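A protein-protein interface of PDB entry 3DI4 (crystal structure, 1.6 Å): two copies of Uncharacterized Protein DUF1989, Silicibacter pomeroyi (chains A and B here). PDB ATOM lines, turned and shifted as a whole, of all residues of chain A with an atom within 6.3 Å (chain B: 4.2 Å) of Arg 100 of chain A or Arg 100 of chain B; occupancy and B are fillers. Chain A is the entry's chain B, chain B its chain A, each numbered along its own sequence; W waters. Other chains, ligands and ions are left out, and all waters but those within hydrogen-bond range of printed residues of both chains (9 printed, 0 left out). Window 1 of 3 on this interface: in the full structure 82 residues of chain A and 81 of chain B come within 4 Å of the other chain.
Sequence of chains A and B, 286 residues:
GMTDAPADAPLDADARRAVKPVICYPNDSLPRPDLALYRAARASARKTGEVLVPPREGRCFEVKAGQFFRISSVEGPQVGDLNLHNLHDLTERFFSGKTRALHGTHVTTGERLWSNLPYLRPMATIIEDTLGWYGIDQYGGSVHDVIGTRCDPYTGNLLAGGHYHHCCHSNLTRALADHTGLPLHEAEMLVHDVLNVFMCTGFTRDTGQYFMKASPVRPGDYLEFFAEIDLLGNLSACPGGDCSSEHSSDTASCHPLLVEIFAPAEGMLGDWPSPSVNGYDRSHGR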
ATOM      1  N   PHE A  95     -12.247  -4.759  28.182  1.00  0.00           N
ATOM      2  CA  PHE A  95     -11.050  -5.021  27.377  1.00  0.00           C
ATOM      3  C   PHE A  95     -10.423  -6.299  27.888  1.00  0.00           C
ATOM      4  O   PHE A  95      -9.621  -6.297  28.824  1.00  0.00           O
ATOM      5  CB  PHE A  95     -10.076  -3.843  27.491  1.00  0.00           C
ATOM      6  CG  PHE A  95      -8.842  -3.892  26.595  1.00  0.00           C
ATOM      7  CD1 PHE A  95      -8.692  -4.781  25.535  1.00  0.00           C
ATOM      8  CD2 PHE A  95      -7.855  -2.933  26.816  1.00  0.00           C
ATOM      9  CE1 PHE A  95      -7.536  -4.738  24.744  1.00  0.00           C
ATOM     10  CE2 PHE A  95      -6.721  -2.902  26.043  1.00  0.00           C
ATOM     11  CZ  PHE A  95      -6.563  -3.794  25.007  1.00  0.00           C
ATOM     12  N   SER A  96     -10.817  -7.418  27.296  1.00  0.00           N
ATOM     13  CA  SER A  96     -10.323  -8.683  27.843  1.00  0.00           C
ATOM     14  C   SER A  96      -8.812  -8.804  27.677  1.00  0.00           C
ATOM     15  O   SER A  96      -8.149  -9.386  28.543  1.00  0.00           O
ATOM     16  CB  SER A  96     -11.038  -9.889  27.257  1.00  0.00           C
ATOM     17  OG  SER A  96     -10.714 -10.064  25.900  1.00  0.00           O
ATOM     18  N   GLY A  97      -8.251  -8.235  26.620  1.00  0.00           N
ATOM     19  CA  GLY A  97      -6.818  -8.388  26.347  1.00  0.00           C
ATOM     20  C   GLY A  97      -5.953  -7.754  27.414  1.00  0.00           C
ATOM     21  O   GLY A  97      -5.014  -8.393  27.887  1.00  0.00           O
ATOM     22  N   LYS A  98      -6.272  -6.534  27.866  1.00  0.00           N
ATOM     23  CA  LYS A  98      -5.426  -5.964  28.951  1.00  0.00           C
ATOM     24  C   LYS A  98      -5.762  -6.619  30.301  1.00  0.00           C
ATOM     25  O   LYS A  98      -4.891  -6.753  31.153  1.00  0.00           O
ATOM     26  CB  LYS A  98      -5.475  -4.425  29.043  1.00  0.00           C
ATOM     27  CG  LYS A  98      -4.085  -3.847  29.451  1.00  0.00           C
ATOM     28  CD  LYS A  98      -3.201  -3.713  28.216  1.00  0.00           C
ATOM     29  CE  LYS A  98      -1.708  -3.754  28.462  1.00  0.00           C
ATOM     30  NZ  LYS A  98      -0.987  -3.464  27.150  1.00  0.00           N
ATOM     31  N   THR A  99      -7.021  -7.002  30.502  1.00  0.00           N
ATOM     32  CA  THR A  99      -7.402  -7.735  31.706  1.00  0.00           C
ATOM     33  C   THR A  99      -6.557  -9.038  31.834  1.00  0.00           C
ATOM     34  O   THR A  99      -6.007  -9.357  32.875  1.00  0.00           O
ATOM     35  CB  THR A  99      -8.880  -8.035  31.683  1.00  0.00           C
ATOM     36  OG1 THR A  99      -9.595  -6.787  31.621  1.00  0.00           O
ATOM     37  CG2 THR A  99      -9.290  -8.810  32.905  1.00  0.00           C
ATOM     38  N   ARG A 100      -6.417  -9.718  30.713  1.00  0.00           N
ATOM     39  CA  ARG A 100      -5.580 -10.910  30.613  1.00  0.00           C
ATOM     40  C   ARG A 100      -4.109 -10.605  30.891  1.00  0.00           C
ATOM     41  O   ARG A 100      -3.436 -11.309  31.643  1.00  0.00           O
ATOM     42  CB  ARG A 100      -5.723 -11.462  29.192  1.00  0.00           C
ATOM     43  CG  ARG A 100      -4.982 -12.771  28.887  1.00  0.00           C
ATOM     44  CD  ARG A 100      -4.853 -13.007  27.411  1.00  0.00           C
ATOM     45  NE  ARG A 100      -6.151 -12.764  26.804  1.00  0.00           N
ATOM     46  CZ  ARG A 100      -6.395 -12.036  25.739  1.00  0.00           C
ATOM     47  NH1 ARG A 100      -5.421 -11.527  24.973  1.00  0.00           N
ATOM     48  NH2 ARG A 100      -7.646 -11.838  25.408  1.00  0.00           N
ATOM     49  N   ALA A 101      -3.593  -9.537  30.297  1.00  0.00           N
ATOM     50  CA  ALA A 101      -2.169  -9.173  30.525  1.00  0.00           C
ATOM     51  C   ALA A 101      -1.900  -8.846  32.010  1.00  0.00           C
ATOM     52  O   ALA A 101      -0.877  -9.225  32.585  1.00  0.00           O
ATOM     53  CB  ALA A 101      -1.786  -7.999  29.614  1.00  0.00           C
ATOM     54  N   LEU A 102      -2.844  -8.161  32.648  1.00  0.00           N
ATOM     55  CA  LEU A 102      -2.676  -7.718  34.038  1.00  0.00           C
ATOM     56  C   LEU A 102      -2.875  -8.854  35.018  1.00  0.00           C
ATOM     57  O   LEU A 102      -2.141  -8.971  36.018  1.00  0.00           O
ATOM     58  CB  LEU A 102      -3.581  -6.502  34.362  1.00  0.00           C
ATOM     59  CG  LEU A 102      -3.260  -5.230  33.567  1.00  0.00           C
ATOM     60  CD1 LEU A 102      -4.287  -4.123  33.872  1.00  0.00           C
ATOM     61  CD2 LEU A 102      -1.816  -4.688  33.829  1.00  0.00           C
ATOM     62  N   HIS A 103      -3.875  -9.694  34.743  1.00  0.00           N
ATOM     63  CA  HIS A 103      -4.303 -10.686  35.723  1.00  0.00           C
ATOM     64  C   HIS A 103      -4.014 -12.146  35.354  1.00  0.00           C
ATOM     65  O   HIS A 103      -3.715 -12.975  36.238  1.00  0.00           O
ATOM     66  CB  HIS A 103      -5.789 -10.550  36.019  1.00  0.00           C
ATOM     67  CG  HIS A 103      -6.160  -9.237  36.628  1.00  0.00           C
ATOM     68  ND1 HIS A 103      -5.559  -8.780  37.784  1.00  0.00           N
ATOM     69  CD2 HIS A 103      -7.070  -8.308  36.267  1.00  0.00           C
ATOM     70  CE1 HIS A 103      -6.088  -7.604  38.093  1.00  0.00           C
ATOM     71  NE2 HIS A 103      -6.987  -7.289  37.174  1.00  0.00           N
ATOM     72  N   GLY A 104      -4.142 -12.477  34.084  1.00  0.00           N
ATOM     73  CA  GLY A 104      -3.841 -13.815  33.590  1.00  0.00           C
ATOM     74  C   GLY A 104      -4.974 -14.332  32.727  1.00  0.00           C
ATOM     75  O   GLY A 104      -5.931 -13.622  32.363  1.00  0.00           O
ATOM     76  N   THR A 105      -4.863 -15.611  32.401  1.00  0.00           N
ATOM     77  CA  THR A 105      -5.812 -16.243  31.480  1.00  0.00           C
ATOM     78  C   THR A 105      -7.256 -16.267  31.953  1.00  0.00           C
ATOM     79  O   THR A 105      -8.169 -16.308  31.129  1.00  0.00           O
ATOM     80  CB  THR A 105      -5.393 -17.693  31.198  1.00  0.00           C
ATOM     81  OG1 THR A 105      -5.299 -18.441  32.417  1.00  0.00           O
ATOM     82  CG2 THR A 105      -4.048 -17.712  30.476  1.00  0.00           C
ATOM     83  N   HIS A 106      -7.426 -16.260  33.270  1.00  0.00           N
ATOM     84  CA  HIS A 106      -8.752 -16.356  33.927  1.00  0.00           C
ATOM     85  C   HIS A 106      -8.751 -15.397  35.120  1.00  0.00           C
ATOM     86  O   HIS A 106      -7.666 -15.027  35.637  1.00  0.00           O
ATOM     87  CB  HIS A 106      -8.988 -17.773  34.426  1.00  0.00           C
ATOM     88  CG  HIS A 106      -8.976 -18.817  33.351  1.00  0.00           C
ATOM     89  ND1 HIS A 106      -7.809 -19.262  32.752  1.00  0.00           N
ATOM     90  CD2 HIS A 106      -9.990 -19.476  32.744  1.00  0.00           C
ATOM     91  CE1 HIS A 106      -8.116 -20.189  31.855  1.00  0.00           C
ATOM     92  NE2 HIS A 106      -9.438 -20.314  31.806  1.00  0.00           N
ATOM     93  N   VAL A 107      -9.936 -14.990  35.560  1.00  0.00           N
ATOM     94  CA  VAL A 107     -10.025 -13.982  36.633  1.00  0.00           C
ATOM     95  C   VAL A 107     -10.787 -14.553  37.830  1.00  0.00           C
ATOM     96  O   VAL A 107     -11.601 -15.469  37.694  1.00  0.00           O
ATOM     97  CB  VAL A 107     -10.641 -12.681  36.166  1.00  0.00           C
ATOM     98  CG1 VAL A 107      -9.643 -12.000  35.238  1.00  0.00           C
ATOM     99  CG2 VAL A 107     -12.000 -12.903  35.497  1.00  0.00           C
ATOM    100  N   VAL A 146     -10.659 -15.154  30.135  1.00  0.00           N
ATOM    101  CA  VAL A 146     -10.437 -13.935  29.378  1.00  0.00           C
ATOM    102  C   VAL A 146      -9.482 -14.211  28.213  1.00  0.00           C
ATOM    103  O   VAL A 146      -8.689 -13.345  27.804  1.00  0.00           O
ATOM    104  CB  VAL A 146     -10.021 -12.741  30.282  1.00  0.00           C
ATOM    105  CG1 VAL A 146     -11.192 -12.385  31.186  1.00  0.00           C
ATOM    106  CG2 VAL A 146      -8.704 -12.987  31.068  1.00  0.00           C
ATOM    107  N   ILE A 147      -9.623 -15.419  27.681  1.00  0.00           N
ATOM    108  CA  ILE A 147      -8.798 -15.873  26.538  1.00  0.00           C
ATOM    109  C   ILE A 147      -9.601 -16.245  25.307  1.00  0.00           C
ATOM    110  O   ILE A 147      -9.037 -16.240  24.213  1.00  0.00           O
ATOM    111  CB  ILE A 147      -7.861 -17.029  26.930  1.00  0.00           C
ATOM    112  CG1 ILE A 147      -8.621 -18.128  27.702  1.00  0.00           C
ATOM    113  CG2 ILE A 147      -6.691 -16.516  27.836  1.00  0.00           C
ATOM    114  CD1 ILE A 147      -7.813 -19.472  27.917  1.00  0.00           C
ATOM    115  N   GLY A 148     -10.900 -16.540  25.456  1.00  0.00           N
ATOM    116  CA  GLY A 148     -11.788 -16.741  24.300  1.00  0.00           C
ATOM    117  C   GLY A 148     -12.285 -15.425  23.743  1.00  0.00           C
ATOM    118  O   GLY A 148     -11.838 -14.312  24.130  1.00  0.00           O
ATOM    119  N   THR A 149     -13.151 -15.508  22.747  1.00  0.00           N
ATOM    120  CA  THR A 149     -13.736 -14.300  22.211  1.00  0.00           C
ATOM    121  C   THR A 149     -15.248 -14.268  22.416  1.00  0.00           C
ATOM    122  O   THR A 149     -15.803 -13.228  22.847  1.00  0.00           O
ATOM    123  CB  THR A 149     -13.401 -14.116  20.703  1.00  0.00           C
ATOM    124  OG1 THR A 149     -13.868 -15.240  19.985  1.00  0.00           O
ATOM    125  CG2 THR A 149     -11.892 -13.941  20.478  1.00  0.00           C
ATOM    126  N   ASP A 193     -14.966  -8.995  23.033  1.00  0.00           N
ATOM    127  CA  ASP A 193     -14.476 -10.240  23.560  1.00  0.00           C
ATOM    128  C   ASP A 193     -14.919 -10.361  25.020  1.00  0.00           C
ATOM    129  O   ASP A 193     -14.820  -9.425  25.802  1.00  0.00           O
ATOM    130  CB  ASP A 193     -12.951 -10.325  23.499  1.00  0.00           C
ATOM    131  CG  ASP A 193     -12.408 -10.435  22.054  1.00  0.00           C
ATOM    132  OD1 ASP A 193     -13.214 -10.452  21.109  1.00  0.00           O
ATOM    133  OD2 ASP A 193     -11.162 -10.514  21.872  1.00  0.00           O
ATOM    134  N   PHE A 203      -5.145 -23.558  27.604  1.00  0.00           N
ATOM    135  CA  PHE A 203      -4.366 -23.863  26.401  1.00  0.00           C
ATOM    136  C   PHE A 203      -3.649 -25.175  26.652  1.00  0.00           C
ATOM    137  O   PHE A 203      -3.073 -25.394  27.728  1.00  0.00           O
ATOM    138  CB  PHE A 203      -3.401 -22.727  26.079  1.00  0.00           C
ATOM    139  CG  PHE A 203      -4.075 -21.455  25.683  1.00  0.00           C
ATOM    140  CD1 PHE A 203      -4.751 -21.389  24.500  1.00  0.00           C
ATOM    141  CD2 PHE A 203      -4.104 -20.358  26.527  1.00  0.00           C
ATOM    142  CE1 PHE A 203      -5.362 -20.215  24.100  1.00  0.00           C
ATOM    143  CE2 PHE A 203      -4.748 -19.195  26.103  1.00  0.00           C
ATOM    144  CZ  PHE A 203      -5.360 -19.161  24.906  1.00  0.00           C
ATOM    145  N   GLY A 208      -0.502 -25.778  22.642  1.00  0.00           N
ATOM    146  CA  GLY A 208      -0.963 -24.404  22.849  1.00  0.00           C
ATOM    147  C   GLY A 208      -2.312 -24.035  22.301  1.00  0.00           C
ATOM    148  O   GLY A 208      -2.570 -22.839  22.063  1.00  0.00           O
ATOM    149  N   GLN A 209      -3.139 -25.041  22.066  1.00  0.00           N
ATOM    150  CA  GLN A 209      -4.458 -24.858  21.511  1.00  0.00           C
ATOM    151  C   GLN A 209      -5.500 -24.603  22.594  1.00  0.00           C
ATOM    152  O   GLN A 209      -5.472 -25.175  23.684  1.00  0.00           O
ATOM    153  CB  GLN A 209      -4.862 -26.077  20.719  1.00  0.00           C
ATOM    154  CG  GLN A 209      -4.058 -26.216  19.452  1.00  0.00           C
ATOM    155  CD  GLN A 209      -4.410 -27.462  18.709  1.00  0.00           C
ATOM    156  OE1 GLN A 209      -5.328 -27.467  17.829  1.00  0.00           O
ATOM    157  NE2 GLN A 209      -3.757 -28.544  19.079  1.00  0.00           N
ATOM    158  N   TYR A 210      -6.462 -23.754  22.258  1.00  0.00           N
ATOM    159  CA  TYR A 210      -7.561 -23.435  23.150  1.00  0.00           C
ATOM    160  C   TYR A 210      -8.473 -24.638  23.341  1.00  0.00           C
ATOM    161  O   TYR A 210      -8.927 -25.234  22.367  1.00  0.00           O
ATOM    162  CB  TYR A 210      -8.330 -22.226  22.594  1.00  0.00           C
ATOM    163  CG  TYR A 210      -9.431 -21.632  23.414  1.00  0.00           C
ATOM    164  CD1 TYR A 210      -9.284 -21.363  24.759  1.00  0.00           C
ATOM    165  CD2 TYR A 210     -10.617 -21.253  22.806  1.00  0.00           C
ATOM    166  CE1 TYR A 210     -10.307 -20.768  25.481  1.00  0.00           C
ATOM    167  CE2 TYR A 210     -11.628 -20.666  23.520  1.00  0.00           C
ATOM    168  CZ  TYR A 210     -11.483 -20.436  24.848  1.00  0.00           C
ATOM    169  OH  TYR A 210     -12.533 -19.827  25.514  1.00  0.00           O
ATOM    170  N   SER B  96      -6.846 -10.887  16.595  1.00  0.00           N
ATOM    171  CA  SER B  96      -5.984 -11.822  17.282  1.00  0.00           C
ATOM    172  C   SER B  96      -6.818 -12.841  18.078  1.00  0.00           C
ATOM    173  O   SER B  96      -6.418 -14.004  18.173  1.00  0.00           O
ATOM    174  CB  SER B  96      -4.951 -11.096  18.141  1.00  0.00           C
ATOM    175  OG  SER B  96      -5.547 -10.500  19.248  1.00  0.00           O
ATOM    176  N   GLY B  97      -7.980 -12.461  18.586  1.00  0.00           N
ATOM    177  CA  GLY B  97      -8.773 -13.381  19.408  1.00  0.00           C
ATOM    178  C   GLY B  97      -9.245 -14.620  18.670  1.00  0.00           C
ATOM    179  O   GLY B  97      -9.075 -15.748  19.165  1.00  0.00           O
ATOM    180  N   LYS B  98      -9.802 -14.453  17.467  1.00  0.00           N
ATOM    181  CA  LYS B  98     -10.234 -15.653  16.740  1.00  0.00           C
ATOM    182  C   LYS B  98      -9.020 -16.423  16.187  1.00  0.00           C
ATOM    183  O   LYS B  98      -9.049 -17.649  16.116  1.00  0.00           O
ATOM    184  CB  LYS B  98     -11.308 -15.406  15.653  1.00  0.00           C
ATOM    185  CG  LYS B  98     -12.304 -16.594  15.529  1.00  0.00           C
ATOM    186  CD  LYS B  98     -13.469 -16.429  16.527  1.00  0.00           C
ATOM    187  CE  LYS B  98     -13.973 -17.724  17.164  1.00  0.00           C
ATOM    188  NZ  LYS B  98     -15.205 -17.445  18.007  1.00  0.00           N
ATOM    189  N   THR B  99      -7.968 -15.732  15.772  1.00  0.00           N
ATOM    190  CA  THR B  99      -6.754 -16.390  15.349  1.00  0.00           C
ATOM    191  C   THR B  99      -6.218 -17.310  16.457  1.00  0.00           C
ATOM    192  O   THR B  99      -5.811 -18.458  16.221  1.00  0.00           O
ATOM    193  CB  THR B  99      -5.726 -15.333  14.965  1.00  0.00           C
ATOM    194  OG1 THR B  99      -6.301 -14.532  13.920  1.00  0.00           O
ATOM    195  CG2 THR B  99      -4.420 -15.943  14.498  1.00  0.00           C
ATOM    196  N   ARG B 100      -6.197 -16.761  17.658  1.00  0.00           N
ATOM    197  CA  ARG B 100      -5.806 -17.527  18.861  1.00  0.00           C
ATOM    198  C   ARG B 100      -6.725 -18.746  19.103  1.00  0.00           C
ATOM    199  O   ARG B 100      -6.245 -19.849  19.372  1.00  0.00           O
ATOM    200  CB  ARG B 100      -5.830 -16.563  20.058  1.00  0.00           C
ATOM    201  CG  ARG B 100      -5.456 -17.185  21.414  1.00  0.00           C
ATOM    202  CD  ARG B 100      -5.891 -16.333  22.610  1.00  0.00           C
ATOM    203  NE  ARG B 100      -5.651 -14.947  22.303  1.00  0.00           N
ATOM    204  CZ  ARG B 100      -6.508 -13.941  22.372  1.00  0.00           C
ATOM    205  NH1 ARG B 100      -7.729 -14.034  22.944  1.00  0.00           N
ATOM    206  NH2 ARG B 100      -6.090 -12.769  21.921  1.00  0.00           N
ATOM    207  N   ALA B 101      -8.042 -18.566  18.982  1.00  0.00           N
ATOM    208  CA  ALA B 101      -8.990 -19.661  19.166  1.00  0.00           C
ATOM    209  C   ALA B 101      -8.770 -20.758  18.142  1.00  0.00           C
ATOM    210  O   ALA B 101      -8.848 -21.945  18.471  1.00  0.00           O
ATOM    211  CB  ALA B 101     -10.484 -19.135  19.106  1.00  0.00           C
ATOM    212  N   LEU B 102      -8.520 -20.363  16.903  1.00  0.00           N
ATOM    213  CA  LEU B 102      -8.402 -21.343  15.814  1.00  0.00           C
ATOM    214  C   LEU B 102      -7.041 -22.030  15.771  1.00  0.00           C
ATOM    215  O   LEU B 102      -6.945 -23.213  15.427  1.00  0.00           O
ATOM    216  CB  LEU B 102      -8.693 -20.723  14.436  1.00  0.00           C
ATOM    217  CG  LEU B 102     -10.121 -20.162  14.214  1.00  0.00           C
ATOM    218  CD1 LEU B 102     -10.207 -19.388  12.851  1.00  0.00           C
ATOM    219  CD2 LEU B 102     -11.194 -21.234  14.307  1.00  0.00           C
ATOM    220  N   HIS B 103      -5.966 -21.302  16.101  1.00  0.00           N
ATOM    221  CA  HIS B 103      -4.607 -21.843  15.977  1.00  0.00           C
ATOM    222  C   HIS B 103      -3.840 -22.045  17.267  1.00  0.00           C
ATOM    223  O   HIS B 103      -3.033 -22.983  17.351  1.00  0.00           O
ATOM    224  CB  HIS B 103      -3.789 -20.934  15.076  1.00  0.00           C
ATOM    225  CG  HIS B 103      -4.366 -20.809  13.702  1.00  0.00           C
ATOM    226  ND1 HIS B 103      -4.570 -21.899  12.880  1.00  0.00           N
ATOM    227  CD2 HIS B 103      -4.719 -19.720  12.981  1.00  0.00           C
ATOM    228  CE1 HIS B 103      -5.044 -21.481  11.716  1.00  0.00           C
ATOM    229  NE2 HIS B 103      -5.146 -20.165  11.755  1.00  0.00           N
ATOM    230  N   GLY B 104      -4.085 -21.189  18.262  1.00  0.00           N
ATOM    231  CA  GLY B 104      -3.392 -21.314  19.529  1.00  0.00           C
ATOM    232  C   GLY B 104      -2.770 -20.022  19.990  1.00  0.00           C
ATOM    233  O   GLY B 104      -2.983 -18.951  19.391  1.00  0.00           O
ATOM    234  N   VAL B 146      -0.123 -14.368  19.818  1.00  0.00           N
ATOM    235  CA  VAL B 146      -1.424 -13.719  19.604  1.00  0.00           C
ATOM    236  C   VAL B 146      -2.196 -13.736  20.926  1.00  0.00           C
ATOM    237  O   VAL B 146      -3.451 -13.889  20.959  1.00  0.00           O
ATOM    238  CB  VAL B 146      -2.231 -14.373  18.475  1.00  0.00           C
ATOM    239  CG1 VAL B 146      -1.541 -14.062  17.132  1.00  0.00           C
ATOM    240  CG2 VAL B 146      -2.420 -15.909  18.700  1.00  0.00           C
ATOM    241  N   ILE B 147      -1.449 -13.523  22.002  1.00  0.00           N
ATOM    242  CA  ILE B 147      -2.016 -13.478  23.371  1.00  0.00           C
ATOM    243  C   ILE B 147      -1.823 -12.141  24.097  1.00  0.00           C
ATOM    244  O   ILE B 147      -2.585 -11.831  25.033  1.00  0.00           O
ATOM    245  CB  ILE B 147      -1.532 -14.695  24.291  1.00  0.00           C
ATOM    246  CG1 ILE B 147      -0.012 -14.825  24.267  1.00  0.00           C
ATOM    247  CG2 ILE B 147      -2.122 -16.003  23.799  1.00  0.00           C
ATOM    248  CD1 ILE B 147       0.560 -15.879  25.198  1.00  0.00           C
ATOM    249  N   PHE B 203       1.970 -18.315  29.141  1.00  0.00           N
ATOM    250  CA  PHE B 203       1.337 -18.158  30.444  1.00  0.00           C
ATOM    251  C   PHE B 203       1.995 -19.087  31.449  1.00  0.00           C
ATOM    252  O   PHE B 203       2.272 -20.250  31.146  1.00  0.00           O
ATOM    253  CB  PHE B 203      -0.168 -18.430  30.351  1.00  0.00           C
ATOM    254  CG  PHE B 203      -0.875 -17.481  29.452  1.00  0.00           C
ATOM    255  CD1 PHE B 203      -1.088 -16.195  29.847  1.00  0.00           C
ATOM    256  CD2 PHE B 203      -1.357 -17.928  28.231  1.00  0.00           C
ATOM    257  CE1 PHE B 203      -1.740 -15.297  28.984  1.00  0.00           C
ATOM    258  CE2 PHE B 203      -2.002 -17.077  27.384  1.00  0.00           C
ATOM    259  CZ  PHE B 203      -2.176 -15.768  27.757  1.00  0.00           C
HETATM  260  O   HOH W   1      -5.316  -9.663  22.782  1.00  0.00           O
HETATM  261  O   HOH W   2      -9.222 -24.464  19.721  1.00  0.00           O
HETATM  262  O   HOH W   3      -6.322 -22.971  19.594  1.00  0.00           O
HETATM  263  O   HOH W   4      -9.880 -16.947  21.392  1.00  0.00           O
HETATM  264  O   HOH W   5      -9.272 -10.195  19.915  1.00  0.00           O
HETATM  265  O   HOH W   6      -9.941 -12.501  23.231  1.00  0.00           O
HETATM  266  O   HOH W   7      -2.738  -9.598  26.824  1.00  0.00           O
HETATM  267  O   HOH W   8     -15.884 -14.442  18.290  1.00  0.00           O
HETATM  268  O   HOH W   9      -6.849 -24.958  17.740  1.00  0.00           O
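The side-chain hydroxyl (OG1) of Thr 149 of chain A lies within hydrogen-bond range of the side-chain amino group (NZ) of Lys 98 of chain B (3.2 Å).
NH2 of Arg 100 of chain A lies close to NH1 of Arg 100 of chain B (3.3 Å).
O of Ile 147 of chain B lies within hydrogen-bond range of NH1 of Arg 100 of chain A (2.9 Å).
The backbone carbonyl oxygen (O) of Ile 147 of chain A sits at hydrogen-bond distance from the guanidinium group (NH1) of Arg 100 of chain B (2.9 Å).
The guanidinium group of Arg 100 of chain A is in hydrogen-bond range of the backbone carbonyl oxygen of Val 146 of chain A, at 2.8 Å.
A ring nitrogen (ND1) of His 106 of chain A is in hydrogen-bond range of the side-chain hydroxyl of Thr 105 of chain A, at 2.7 Å.
The guanidinium group of Arg 100 of chain B lies within hydrogen-bond range of the backbone carbonyl oxygen of Val 146 of chain B (2.8 Å).
O of Thr 105 of chain A lies within hydrogen-bond range of N of Val 146 of chain A (2.9 Å).
Phe 203 of chain B touches Arg 100 of chain A (CZ to CD, 3.9 Å).
Phe 203 of chain B touches Thr 105 of chain A (CG to CG2, 3.3 Å).
Gly 97 of chain B touches Thr 149 of chain A (C to CG2, 3.3 Å).
Arg 100 of chain B touches Phe 203 of chain A.
CE2 of Phe 203 of chain B touches CE2 of Phe 203 of chain A, 3.7 Å away.
O of Gly 208 of chain A touches CA of Gly 104 of chain B (3.1 Å).
Gln 209 of chain A touches His 103 of chain B (CG to O, 3.99 Å).
Water W4 lies within hydrogen-bond range of O of Gly 97 of chain B (2.7 Å), O of Ile 147 of chain A (3.0 Å) and N of Ala 101 of chain B (3.4 Å).
Water W5 lies within hydrogen-bond range of the side-chain carboxylate of Asp 193 of chain A and the backbone NH of Gly 97 of chain B.
Water W2 lies within hydrogen-bond range of O of Tyr 210 of chain A and O of Ala 101 of chain B.
Water W3 lies within hydrogen-bond range of the backbone NH (N) of Tyr 210 of chain A (2.8 Å), the backbone carbonyl oxygen (O) of Ala 101 of chain B (2.9 Å), the backbone carbonyl oxygen (O) of Arg 100 of chain B (3.1 Å) and the backbone NH (N) of Gly 104 of chain B (3.2 Å).
Water W1 lies within hydrogen-bond range of NH1 of Arg 100 of chain A (2.9 Å) and NH2 of Arg 100 of chain B (3.3 Å).
Water W9 lies within hydrogen-bond range of the backbone carbonyl oxygen of Leu 102 of chain B (2.9 Å) and the side-chain amide oxygen of Gln 209 of chain A (2.9 Å).
Of the 12 printed residues of chain B, 7 touch a printed residue of chain A.
Along chain B the printed residues that touch a printed residue of chain A span positions 97 to 203.
Of the 22 printed residues of chain A, 7 touch a printed residue of chain B.
Printed residues of chain A that touch a printed residue of chain B: Arg 100, Thr 105, Ile 147, Thr 149, Phe 203, Gly 208 and Gln 209.
Hydrophobic or aromatic side chains of chain A that line the printed part of chain B: Phe 203.
Among the printed residues, no Asp or Glu carboxylate lies within 4 Å of a Lys or Arg side-chain nitrogen of the other chain.
Arg 100 of chain B touches its own counterpart, Arg 100 of chain A.
Arg 100 of chain A touches Ile 147 of chain B, and with the chains exchanged Ile 147 of chain A touches Arg 100 of chain B.
Arg 100 of chain A touches Phe 203 of chain B, and with the chains exchanged Phe 203 of chain A touches Arg 100 of chain B.
Phe 203 of chain A touches its own counterpart, Phe 203 of chain B.
Of the 11 pairs that touch across the chains among the printed residues, 6 have their exchanged pair printed and touching as well.
Arg 100 of chain A touches just these residues of chain B: Arg 100, Ile 147 and Phe 203.
Of the printed residues of chain A, Arg 100 of chain B touches Arg 100, Ile 147 and Phe 203.
Of the printed residues of chain A, Gly 97 of chain B touches Thr 149 (3.3 Å).
Of the printed residues of chain B, Thr 149 of chain A touches Gly 97 (3.3 Å) and Lys 98 (3.2 Å).
Printed residues of chain A within 4 Å of Gly 104 of chain B: Gly 208.
The nearest residue of chain A that does not touch Arg 100 of chain B is Gly 148 of chain A (4.3 Å).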
